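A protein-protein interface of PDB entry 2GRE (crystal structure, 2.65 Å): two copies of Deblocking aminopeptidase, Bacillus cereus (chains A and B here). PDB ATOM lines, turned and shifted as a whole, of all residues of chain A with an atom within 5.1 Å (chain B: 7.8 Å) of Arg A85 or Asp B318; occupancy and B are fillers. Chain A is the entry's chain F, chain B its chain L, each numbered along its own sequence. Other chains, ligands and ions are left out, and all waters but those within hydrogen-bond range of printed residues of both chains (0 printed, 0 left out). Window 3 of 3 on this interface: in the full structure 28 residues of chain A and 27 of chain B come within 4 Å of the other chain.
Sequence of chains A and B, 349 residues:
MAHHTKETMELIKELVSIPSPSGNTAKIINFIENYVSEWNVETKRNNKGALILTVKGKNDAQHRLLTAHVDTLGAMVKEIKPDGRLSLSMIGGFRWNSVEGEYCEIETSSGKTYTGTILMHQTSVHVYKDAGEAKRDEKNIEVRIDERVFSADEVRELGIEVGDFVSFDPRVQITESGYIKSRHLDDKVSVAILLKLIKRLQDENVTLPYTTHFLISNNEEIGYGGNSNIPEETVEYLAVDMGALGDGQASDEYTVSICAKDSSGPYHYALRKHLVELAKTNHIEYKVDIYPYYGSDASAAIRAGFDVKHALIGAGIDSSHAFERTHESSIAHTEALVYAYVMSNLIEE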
ATOM      1  N   GLU A  79     -20.799 -16.127  24.334  1.00  0.00           N
ATOM      2  CA  GLU A  79     -20.298 -17.118  23.394  1.00  0.00           C
ATOM      3  C   GLU A  79     -19.085 -17.865  23.933  1.00  0.00           C
ATOM      4  O   GLU A  79     -18.251 -17.314  24.667  1.00  0.00           O
ATOM      5  CB  GLU A  79     -19.971 -16.467  22.043  1.00  0.00           C
ATOM      6  CG  GLU A  79     -19.446 -17.425  20.983  1.00  0.00           C
ATOM      7  CD  GLU A  79     -19.080 -16.726  19.699  1.00  0.00           C
ATOM      8  OE1 GLU A  79     -19.738 -15.710  19.364  1.00  0.00           O
ATOM      9  OE2 GLU A  79     -18.144 -17.196  19.012  1.00  0.00           O
ATOM     10  N   ILE A  80     -18.982 -19.130  23.540  1.00  0.00           N
ATOM     11  CA  ILE A  80     -17.804 -19.910  23.885  1.00  0.00           C
ATOM     12  C   ILE A  80     -16.866 -20.019  22.708  1.00  0.00           C
ATOM     13  O   ILE A  80     -17.110 -20.782  21.767  1.00  0.00           O
ATOM     14  CB  ILE A  80     -18.160 -21.276  24.479  1.00  0.00           C
ATOM     15  CG1 ILE A  80     -18.634 -21.078  25.904  1.00  0.00           C
ATOM     16  CG2 ILE A  80     -16.954 -22.150  24.539  1.00  0.00           C
ATOM     17  CD1 ILE A  80     -19.146 -22.331  26.517  1.00  0.00           C
ATOM     18  N   LYS A  81     -15.791 -19.242  22.769  1.00  0.00           N
ATOM     19  CA  LYS A  81     -14.867 -19.150  21.659  1.00  0.00           C
ATOM     20  C   LYS A  81     -14.107 -20.474  21.424  1.00  0.00           C
ATOM     21  O   LYS A  81     -13.901 -21.236  22.376  1.00  0.00           O
ATOM     22  CB  LYS A  81     -13.936 -17.959  21.861  1.00  0.00           C
ATOM     23  CG  LYS A  81     -14.695 -16.640  21.821  1.00  0.00           C
ATOM     24  CD  LYS A  81     -13.833 -15.477  21.335  1.00  0.00           C
ATOM     25  CE  LYS A  81     -13.120 -14.803  22.498  1.00  0.00           C
ATOM     26  NZ  LYS A  81     -12.479 -13.548  22.057  1.00  0.00           N
ATOM     27  N   ASP A  83     -11.021 -21.151  21.024  1.00  0.00           N
ATOM     28  CA  ASP A  83      -9.851 -21.241  21.889  1.00  0.00           C
ATOM     29  C   ASP A  83     -10.180 -21.462  23.363  1.00  0.00           C
ATOM     30  O   ASP A  83      -9.287 -21.657  24.151  1.00  0.00           O
ATOM     31  CB  ASP A  83      -8.985 -19.978  21.744  1.00  0.00           C
ATOM     32  CG  ASP A  83      -9.547 -18.747  22.517  1.00  0.00           C
ATOM     33  OD1 ASP A  83      -8.742 -17.846  22.852  1.00  0.00           O
ATOM     34  OD2 ASP A  83     -10.770 -18.655  22.793  1.00  0.00           O
ATOM     35  N   GLY A  84     -11.447 -21.376  23.759  1.00  0.00           N
ATOM     36  CA  GLY A  84     -11.820 -21.664  25.151  1.00  0.00           C
ATOM     37  C   GLY A  84     -11.858 -20.455  26.052  1.00  0.00           C
ATOM     38  O   GLY A  84     -12.055 -20.565  27.248  1.00  0.00           O
ATOM     39  N   ARG A  85     -11.657 -19.284  25.477  1.00  0.00           N
ATOM     40  CA  ARG A  85     -11.884 -18.062  26.226  1.00  0.00           C
ATOM     41  C   ARG A  85     -13.333 -17.654  25.989  1.00  0.00           C
ATOM     42  O   ARG A  85     -13.978 -18.128  25.041  1.00  0.00           O
ATOM     43  CB  ARG A  85     -10.879 -16.970  25.859  1.00  0.00           C
ATOM     44  CG  ARG A  85      -9.464 -17.237  26.444  1.00  0.00           C
ATOM     45  CD  ARG A  85      -8.456 -16.107  26.172  1.00  0.00           C
ATOM     46  NE  ARG A  85      -7.146 -16.368  26.785  1.00  0.00           N
ATOM     47  CZ  ARG A  85      -6.108 -15.521  26.780  1.00  0.00           C
ATOM     48  NH1 ARG A  85      -6.179 -14.325  26.197  1.00  0.00           N
ATOM     49  NH2 ARG A  85      -4.976 -15.867  27.370  1.00  0.00           N
ATOM     50  N   LEU A  86     -13.854 -16.815  26.879  1.00  0.00           N
ATOM     51  CA  LEU A  86     -15.261 -16.453  26.887  1.00  0.00           C
ATOM     52  C   LEU A  86     -15.493 -15.068  26.340  1.00  0.00           C
ATOM     53  O   LEU A  86     -14.795 -14.107  26.689  1.00  0.00           O
ATOM     54  CB  LEU A  86     -15.776 -16.472  28.304  1.00  0.00           C
ATOM     55  CG  LEU A  86     -16.361 -17.751  28.859  1.00  0.00           C
ATOM     56  CD1 LEU A  86     -15.869 -18.928  28.100  1.00  0.00           C
ATOM     57  CD2 LEU A  86     -16.015 -17.835  30.339  1.00  0.00           C
ATOM     58  N   SER A  87     -16.483 -14.990  25.466  1.00  0.00           N
ATOM     59  CA  SER A  87     -17.013 -13.733  24.995  1.00  0.00           C
ATOM     60  C   SER A  87     -18.010 -13.232  26.062  1.00  0.00           C
ATOM     61  O   SER A  87     -18.599 -14.039  26.804  1.00  0.00           O
ATOM     62  CB  SER A  87     -17.727 -14.001  23.694  1.00  0.00           C
ATOM     63  OG  SER A  87     -17.618 -12.891  22.857  1.00  0.00           O
ATOM     64  N   LEU A 119      -9.978  -9.483  29.740  1.00  0.00           N
ATOM     65  CA  LEU A 119      -8.928  -8.834  28.952  1.00  0.00           C
ATOM     66  C   LEU A 119      -9.483  -8.415  27.613  1.00  0.00           C
ATOM     67  O   LEU A 119     -10.458  -9.002  27.153  1.00  0.00           O
ATOM     68  CB  LEU A 119      -7.755  -9.794  28.730  1.00  0.00           C
ATOM     69  CG  LEU A 119      -7.228 -10.649  29.885  1.00  0.00           C
ATOM     70  CD1 LEU A 119      -6.624 -11.923  29.338  1.00  0.00           C
ATOM     71  CD2 LEU A 119      -6.228  -9.878  30.764  1.00  0.00           C
ATOM     72  N   GLU A 142     -13.029 -10.264  26.738  1.00  0.00           N
ATOM     73  CA  GLU A 142     -13.045 -11.718  26.946  1.00  0.00           C
ATOM     74  C   GLU A 142     -12.572 -12.090  28.334  1.00  0.00           C
ATOM     75  O   GLU A 142     -11.893 -11.289  29.013  1.00  0.00           O
ATOM     76  CB  GLU A 142     -12.120 -12.421  25.937  1.00  0.00           C
ATOM     77  CG  GLU A 142     -10.648 -12.510  26.391  1.00  0.00           C
ATOM     78  CD  GLU A 142      -9.671 -12.858  25.273  1.00  0.00           C
ATOM     79  OE1 GLU A 142     -10.100 -13.158  24.140  1.00  0.00           O
ATOM     80  OE2 GLU A 142      -8.456 -12.820  25.536  1.00  0.00           O
ATOM     81  N   VAL A 143     -12.886 -13.331  28.709  1.00  0.00           N
ATOM     82  CA  VAL A 143     -12.409 -13.950  29.940  1.00  0.00           C
ATOM     83  C   VAL A 143     -11.387 -15.045  29.706  1.00  0.00           C
ATOM     84  O   VAL A 143     -11.688 -16.024  29.066  1.00  0.00           O
ATOM     85  CB  VAL A 143     -13.556 -14.613  30.691  1.00  0.00           C
ATOM     86  CG1 VAL A 143     -13.067 -15.130  32.056  1.00  0.00           C
ATOM     87  CG2 VAL A 143     -14.678 -13.643  30.823  1.00  0.00           C
ATOM     88  N   ARG A 144     -10.194 -14.881  30.255  1.00  0.00           N
ATOM     89  CA  ARG A 144      -9.216 -15.953  30.306  1.00  0.00           C
ATOM     90  C   ARG A 144      -9.441 -16.739  31.595  1.00  0.00           C
ATOM     91  O   ARG A 144      -9.243 -16.203  32.688  1.00  0.00           O
ATOM     92  CB  ARG A 144      -7.805 -15.365  30.175  1.00  0.00           C
ATOM     93  CG  ARG A 144      -6.630 -16.226  30.600  1.00  0.00           C
ATOM     94  CD  ARG A 144      -6.000 -15.568  31.813  1.00  0.00           C
ATOM     95  NE  ARG A 144      -4.794 -14.823  31.469  1.00  0.00           N
ATOM     96  CZ  ARG A 144      -4.256 -13.834  32.186  1.00  0.00           C
ATOM     97  NH1 ARG A 144      -4.815 -13.409  33.308  1.00  0.00           N
ATOM     98  NH2 ARG A 144      -3.135 -13.264  31.760  1.00  0.00           N
ATOM     99  N   ILE A 145      -9.891 -17.996  31.446  1.00  0.00           N
ATOM    100  CA  ILE A 145     -10.380 -18.805  32.576  1.00  0.00           C
ATOM    101  C   ILE A 145      -9.221 -19.468  33.271  1.00  0.00           C
ATOM    102  O   ILE A 145      -8.301 -19.921  32.626  1.00  0.00           O
ATOM    103  CB  ILE A 145     -11.358 -19.919  32.134  1.00  0.00           C
ATOM    104  CG1 ILE A 145     -12.609 -19.336  31.454  1.00  0.00           C
ATOM    105  CG2 ILE A 145     -11.781 -20.770  33.324  1.00  0.00           C
ATOM    106  CD1 ILE A 145     -13.631 -20.388  30.955  1.00  0.00           C
ATOM    107  N   ILE B 180      -0.589 -18.915  38.525  1.00  0.00           N
ATOM    108  CA  ILE B 180      -0.312 -17.774  39.359  1.00  0.00           C
ATOM    109  C   ILE B 180      -0.619 -16.516  38.542  1.00  0.00           C
ATOM    110  O   ILE B 180       0.028 -16.255  37.518  1.00  0.00           O
ATOM    111  CB  ILE B 180       1.140 -17.810  39.912  1.00  0.00           C
ATOM    112  CG1 ILE B 180       1.412 -16.592  40.794  1.00  0.00           C
ATOM    113  CG2 ILE B 180       2.164 -17.899  38.791  1.00  0.00           C
ATOM    114  CD1 ILE B 180       2.731 -16.652  41.559  1.00  0.00           C
ATOM    115  N   LEU B 185       5.007 -10.280  38.470  1.00  0.00           N
ATOM    116  CA  LEU B 185       5.692 -11.296  37.736  1.00  0.00           C
ATOM    117  C   LEU B 185       6.529 -10.420  36.828  1.00  0.00           C
ATOM    118  O   LEU B 185       6.642  -9.180  37.029  1.00  0.00           O
ATOM    119  CB  LEU B 185       4.706 -12.155  36.918  1.00  0.00           C
ATOM    120  CG  LEU B 185       3.460 -12.765  37.573  1.00  0.00           C
ATOM    121  CD1 LEU B 185       2.831 -13.796  36.684  1.00  0.00           C
ATOM    122  CD2 LEU B 185       3.748 -13.395  38.915  1.00  0.00           C
ATOM    123  N   MET B 242      11.194 -13.281  30.814  1.00  0.00           N
ATOM    124  CA  MET B 242       9.985 -13.716  30.114  1.00  0.00           C
ATOM    125  C   MET B 242       9.486 -12.589  29.257  1.00  0.00           C
ATOM    126  O   MET B 242       9.406 -11.476  29.745  1.00  0.00           O
ATOM    127  CB  MET B 242       8.878 -14.126  31.113  1.00  0.00           C
ATOM    128  CG  MET B 242       9.307 -14.978  32.351  1.00  0.00           C
ATOM    129  SD  MET B 242       7.911 -15.277  33.795  1.00  0.00           S
ATOM    130  CE  MET B 242       7.294 -13.432  34.042  1.00  0.00           C
ATOM    131  N   GLY B 243       9.141 -12.879  27.995  1.00  0.00           N
ATOM    132  CA  GLY B 243       8.553 -11.872  27.070  1.00  0.00           C
ATOM    133  C   GLY B 243       7.194 -12.183  26.416  1.00  0.00           C
ATOM    134  O   GLY B 243       6.632 -13.259  26.625  1.00  0.00           O
ATOM    135  N   ALA B 244       6.681 -11.228  25.623  1.00  0.00           N
ATOM    136  CA  ALA B 244       5.426 -11.340  24.845  1.00  0.00           C
ATOM    137  C   ALA B 244       5.665 -11.749  23.352  1.00  0.00           C
ATOM    138  O   ALA B 244       6.824 -11.873  22.942  1.00  0.00           O
ATOM    139  CB  ALA B 244       4.682 -10.011  24.921  1.00  0.00           C
ATOM    140  N   ASP B 247       1.062 -13.377  19.271  1.00  0.00           N
ATOM    141  CA  ASP B 247       0.409 -14.696  19.099  1.00  0.00           C
ATOM    142  C   ASP B 247      -0.044 -15.270  20.464  1.00  0.00           C
ATOM    143  O   ASP B 247      -0.534 -14.519  21.303  1.00  0.00           O
ATOM    144  CB  ASP B 247       1.408 -15.680  18.468  1.00  0.00           C
ATOM    145  CG  ASP B 247       1.689 -15.390  17.009  1.00  0.00           C
ATOM    146  OD1 ASP B 247       0.829 -14.743  16.350  1.00  0.00           O
ATOM    147  OD2 ASP B 247       2.760 -15.827  16.526  1.00  0.00           O
ATOM    148  N   GLY B 248       0.146 -16.584  20.690  1.00  0.00           N
ATOM    149  CA  GLY B 248      -0.258 -17.279  21.935  1.00  0.00           C
ATOM    150  C   GLY B 248       0.703 -17.140  23.113  1.00  0.00           C
ATOM    151  O   GLY B 248       0.500 -17.727  24.188  1.00  0.00           O
ATOM    152  N   ASP B 252       2.402 -19.327  25.551  1.00  0.00           N
ATOM    153  CA  ASP B 252       2.054 -20.704  25.986  1.00  0.00           C
ATOM    154  C   ASP B 252       2.506 -20.939  27.420  1.00  0.00           C
ATOM    155  O   ASP B 252       3.692 -21.028  27.697  1.00  0.00           O
ATOM    156  CB  ASP B 252       2.626 -21.763  25.022  1.00  0.00           C
ATOM    157  CG  ASP B 252       2.558 -23.201  25.575  1.00  0.00           C
ATOM    158  OD1 ASP B 252       1.824 -23.467  26.542  1.00  0.00           O
ATOM    159  OD2 ASP B 252       3.243 -24.094  25.030  1.00  0.00           O
ATOM    160  N   GLU B 253       1.537 -21.053  28.323  1.00  0.00           N
ATOM    161  CA  GLU B 253       1.797 -20.988  29.758  1.00  0.00           C
ATOM    162  C   GLU B 253       2.243 -22.306  30.377  1.00  0.00           C
ATOM    163  O   GLU B 253       2.502 -22.369  31.582  1.00  0.00           O
ATOM    164  CB  GLU B 253       0.568 -20.457  30.495  1.00  0.00           C
ATOM    165  CG  GLU B 253      -0.023 -19.183  29.909  1.00  0.00           C
ATOM    166  CD  GLU B 253      -1.148 -18.622  30.762  1.00  0.00           C
ATOM    167  OE1 GLU B 253      -2.314 -18.576  30.311  1.00  0.00           O
ATOM    168  OE2 GLU B 253      -0.874 -18.246  31.919  1.00  0.00           O
ATOM    169  N   TYR B 254       2.369 -23.351  29.564  1.00  0.00           N
ATOM    170  CA  TYR B 254       2.558 -24.707  30.080  1.00  0.00           C
ATOM    171  C   TYR B 254       3.876 -25.326  29.715  1.00  0.00           C
ATOM    172  O   TYR B 254       4.072 -26.532  29.894  1.00  0.00           O
ATOM    173  CB  TYR B 254       1.411 -25.586  29.600  1.00  0.00           C
ATOM    174  CG  TYR B 254       0.107 -24.873  29.753  1.00  0.00           C
ATOM    175  CD1 TYR B 254      -0.482 -24.230  28.657  1.00  0.00           C
ATOM    176  CD2 TYR B 254      -0.514 -24.790  30.995  1.00  0.00           C
ATOM    177  CE1 TYR B 254      -1.674 -23.539  28.781  1.00  0.00           C
ATOM    178  CE2 TYR B 254      -1.717 -24.098  31.145  1.00  0.00           C
ATOM    179  CZ  TYR B 254      -2.296 -23.463  30.031  1.00  0.00           C
ATOM    180  OH  TYR B 254      -3.496 -22.792  30.142  1.00  0.00           O
ATOM    181  N   ALA B 315       9.811 -18.937  31.613  1.00  0.00           N
ATOM    182  CA  ALA B 315       8.466 -19.498  31.571  1.00  0.00           C
ATOM    183  C   ALA B 315       7.610 -18.656  30.651  1.00  0.00           C
ATOM    184  O   ALA B 315       7.898 -17.462  30.414  1.00  0.00           O
ATOM    185  CB  ALA B 315       7.863 -19.535  32.941  1.00  0.00           C
ATOM    186  N   GLY B 316       6.581 -19.291  30.101  1.00  0.00           N
ATOM    187  CA  GLY B 316       5.661 -18.642  29.188  1.00  0.00           C
ATOM    188  C   GLY B 316       4.700 -17.817  30.001  1.00  0.00           C
ATOM    189  O   GLY B 316       4.169 -18.269  31.013  1.00  0.00           O
ATOM    190  N   ILE B 317       4.506 -16.576  29.600  1.00  0.00           N
ATOM    191  CA  ILE B 317       3.575 -15.758  30.327  1.00  0.00           C
ATOM    192  C   ILE B 317       2.692 -15.013  29.395  1.00  0.00           C
ATOM    193  O   ILE B 317       3.133 -14.378  28.448  1.00  0.00           O
ATOM    194  CB  ILE B 317       4.251 -14.917  31.483  1.00  0.00           C
ATOM    195  CG1 ILE B 317       4.364 -13.412  31.223  1.00  0.00           C
ATOM    196  CG2 ILE B 317       5.583 -15.556  31.860  1.00  0.00           C
ATOM    197  CD1 ILE B 317       5.533 -13.019  30.389  1.00  0.00           C
ATOM    198  N   ASP B 318       1.421 -15.164  29.674  1.00  0.00           N
ATOM    199  CA  ASP B 318       0.349 -14.621  28.906  1.00  0.00           C
ATOM    200  C   ASP B 318       0.078 -13.201  29.361  1.00  0.00           C
ATOM    201  O   ASP B 318       0.160 -12.906  30.556  1.00  0.00           O
ATOM    202  CB  ASP B 318      -0.850 -15.501  29.192  1.00  0.00           C
ATOM    203  CG  ASP B 318      -2.024 -15.140  28.383  1.00  0.00           C
ATOM    204  OD1 ASP B 318      -2.565 -14.050  28.616  1.00  0.00           O
ATOM    205  OD2 ASP B 318      -2.430 -15.959  27.536  1.00  0.00           O
ATOM    206  N   SER B 319      -0.252 -12.331  28.399  1.00  0.00           N
ATOM    207  CA  SER B 319      -0.671 -10.925  28.661  1.00  0.00           C
ATOM    208  C   SER B 319       0.463 -10.112  29.327  1.00  0.00           C
ATOM    209  O   SER B 319       0.243  -9.173  30.094  1.00  0.00           O
ATOM    210  CB  SER B 319      -2.004 -10.899  29.461  1.00  0.00           C
ATOM    211  OG  SER B 319      -2.446  -9.594  29.829  1.00  0.00           O
ATOM    212  N   SER B 320       1.687 -10.508  29.020  1.00  0.00           N
ATOM    213  CA  SER B 320       2.898  -9.828  29.490  1.00  0.00           C
ATOM    214  C   SER B 320       2.803  -8.300  29.653  1.00  0.00           C
ATOM    215  O   SER B 320       2.400  -7.594  28.700  1.00  0.00           O
ATOM    216  CB  SER B 320       4.054 -10.124  28.525  1.00  0.00           C
ATOM    217  OG  SER B 320       5.125  -9.220  28.740  1.00  0.00           O
ATOM    218  N   HIS B 321       3.206  -7.823  30.849  1.00  0.00           N
ATOM    219  CA  HIS B 321       3.348  -6.390  31.229  1.00  0.00           C
ATOM    220  C   HIS B 321       2.027  -5.661  31.536  1.00  0.00           C
ATOM    221  O   HIS B 321       2.039  -4.600  32.162  1.00  0.00           O
ATOM    222  CB  HIS B 321       4.225  -5.586  30.227  1.00  0.00           C
ATOM    223  N   ALA B 322       0.910  -6.214  31.061  1.00  0.00           N
ATOM    224  CA  ALA B 322      -0.414  -5.854  31.558  1.00  0.00           C
ATOM    225  C   ALA B 322      -0.721  -6.808  32.726  1.00  0.00           C
ATOM    226  O   ALA B 322      -0.160  -6.659  33.825  1.00  0.00           O
ATOM    227  CB  ALA B 322      -1.470  -5.951  30.444  1.00  0.00           C
ATOM    228  N   PHE B 323      -1.552  -7.821  32.484  1.00  0.00           N
ATOM    229  CA  PHE B 323      -2.008  -8.672  33.569  1.00  0.00           C
ATOM    230  C   PHE B 323      -1.441 -10.061  33.391  1.00  0.00           C
ATOM    231  O   PHE B 323      -1.794 -10.787  32.461  1.00  0.00           O
ATOM    232  CB  PHE B 323      -3.510  -8.637  33.586  1.00  0.00           C
ATOM    233  CG  PHE B 323      -4.057  -7.260  33.289  1.00  0.00           C
ATOM    234  CD1 PHE B 323      -4.429  -6.914  31.992  1.00  0.00           C
ATOM    235  CD2 PHE B 323      -4.144  -6.304  34.303  1.00  0.00           C
ATOM    236  CE1 PHE B 323      -4.903  -5.652  31.717  1.00  0.00           C
ATOM    237  CE2 PHE B 323      -4.636  -5.044  34.059  1.00  0.00           C
ATOM    238  CZ  PHE B 323      -5.019  -4.700  32.763  1.00  0.00           C
ATOM    239  N   GLU B 324      -0.519 -10.414  34.273  1.00  0.00           N
ATOM    240  CA  GLU B 324       0.360 -11.506  33.971  1.00  0.00           C
ATOM    241  C   GLU B 324      -0.161 -12.825  34.577  1.00  0.00           C
ATOM    242  O   GLU B 324      -0.782 -12.836  35.656  1.00  0.00           O
ATOM    243  CB  GLU B 324       1.811 -11.143  34.360  1.00  0.00           C
ATOM    244  CG  GLU B 324       2.305  -9.781  33.789  1.00  0.00           C
ATOM    245  CD  GLU B 324       3.819  -9.558  33.918  1.00  0.00           C
ATOM    246  OE1 GLU B 324       4.527 -10.358  34.562  1.00  0.00           O
ATOM    247  OE2 GLU B 324       4.345  -8.576  33.366  1.00  0.00           O
ATOM    248  N   ARG B 325       0.032 -13.909  33.832  1.00  0.00           N
ATOM    249  CA  ARG B 325      -0.316 -15.231  34.291  1.00  0.00           C
ATOM    250  C   ARG B 325       0.650 -16.299  33.761  1.00  0.00           C
ATOM    251  O   ARG B 325       1.078 -16.266  32.606  1.00  0.00           O
ATOM    252  CB  ARG B 325      -1.752 -15.601  33.913  1.00  0.00           C
ATOM    253  CG  ARG B 325      -2.278 -16.777  34.705  1.00  0.00           C
ATOM    254  CD  ARG B 325      -3.703 -17.237  34.335  1.00  0.00           C
ATOM    255  NE  ARG B 325      -3.775 -17.918  33.048  1.00  0.00           N
ATOM    256  CZ  ARG B 325      -4.812 -18.615  32.592  1.00  0.00           C
ATOM    257  NH1 ARG B 325      -5.921 -18.778  33.304  1.00  0.00           N
ATOM    258  NH2 ARG B 325      -4.737 -19.152  31.393  1.00  0.00           N
ATOM    259  N   THR B 326       1.014 -17.249  34.611  1.00  0.00           N
ATOM    260  CA  THR B 326       1.626 -18.449  34.075  1.00  0.00           C
ATOM    261  C   THR B 326       1.046 -19.631  34.809  1.00  0.00           C
ATOM    262  O   THR B 326       0.225 -19.449  35.715  1.00  0.00           O
ATOM    263  CB  THR B 326       3.198 -18.399  34.011  1.00  0.00           C
ATOM    264  OG1 THR B 326       3.678 -19.562  33.335  1.00  0.00           O
ATOM    265  CG2 THR B 326       3.855 -18.310  35.376  1.00  0.00           C
ATOM    266  N   HIS B 327       1.416 -20.832  34.389  1.00  0.00           N
ATOM    267  CA  HIS B 327       0.945 -22.042  35.053  1.00  0.00           C
ATOM    268  C   HIS B 327       2.098 -22.804  35.638  1.00  0.00           C
ATOM    269  O   HIS B 327       3.203 -22.770  35.082  1.00  0.00           O
ATOM    270  CB  HIS B 327       0.218 -22.947  34.094  1.00  0.00           C
ATOM    271  CG  HIS B 327      -0.390 -24.106  34.775  1.00  0.00           C
ATOM    272  ND1 HIS B 327       0.174 -25.359  34.746  1.00  0.00           N
ATOM    273  CD2 HIS B 327      -1.483 -24.196  35.570  1.00  0.00           C
ATOM    274  CE1 HIS B 327      -0.572 -26.181  35.463  1.00  0.00           C
ATOM    275  NE2 HIS B 327      -1.581 -25.500  35.978  1.00  0.00           N
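O of Phe B323 lies within hydrogen-bond range of NH2 of Arg A144. O of Ile A145 is in hydrogen-bond range of NH1 of Arg B325 (2.7 Å). The guanidinium group (NH2) of Arg A85 lies within salt-bridge range of the side-chain carboxylate (OD2) of Asp B318 (2.6 Å). NH2 of Arg A144 lies within salt-bridge range of OD1 of Asp B318 (3.3 Å).
The side-chain hydroxyl (OG) of Ser B319 sits at hydrogen-bond distance from the backbone carbonyl oxygen (O) of Phe B323 (3.0 Å). The guanidinium group (NH1) of Arg A85 is in salt-bridge range of the side-chain carboxylate (OE2) of Glu A142 (2.8 Å). The backbone NH (N) of Leu A119 is in hydrogen-bond range of the backbone carbonyl oxygen (O) of Glu A142, at 2.7 Å. The guanidinium group (NH2) of Arg B325 is in salt-bridge range of the side-chain carboxylate (OE1) of Glu B253, at 2.7 Å. The backbone NH of Asp B318 is in hydrogen-bond range of the backbone carbonyl oxygen of Arg B325 (3.2 Å). N of Arg A85 sits at hydrogen-bond distance from OD2 of Asp A83 (2.9 Å).
Among the printed residues, pairs that only touch across the chains: Arg A144 with Arg B325, Arg A144 with Ser B319, Leu A119 with Phe B323 and Leu A119 with Ser B319.
Asp B318 touches just these residues of chain A: Arg A85 (2.6 Å) and Arg A144 (3.3 Å). Of the printed residues of chain A, Ser B319 touches Leu A119 (3.9 Å) and Arg A144 (3.5 Å). Printed residues of chain A within 4 Å of Arg B325: Arg A144 and Ile A145. The nearest residue of chain B that does not touch Arg A85 is Glu B253 (4.8 Å). The nearest residue of chain A that does not touch Asp B318 is Leu A119 (4.6 Å).
Of the 13 printed residues of chain A, 4 touch a printed residue of chain B. Hydrophobic or aromatic side chains of chain A that line the printed part of chain B: Leu A119. Among the printed residues, Asp or Glu carboxylates within 4 Å of a Lys or Arg side-chain nitrogen of the other chain: Arg A85 with Asp B318 (2.6 Å) and Arg A144 with Asp B318 (3.3 Å).
No position is printed for both chains.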
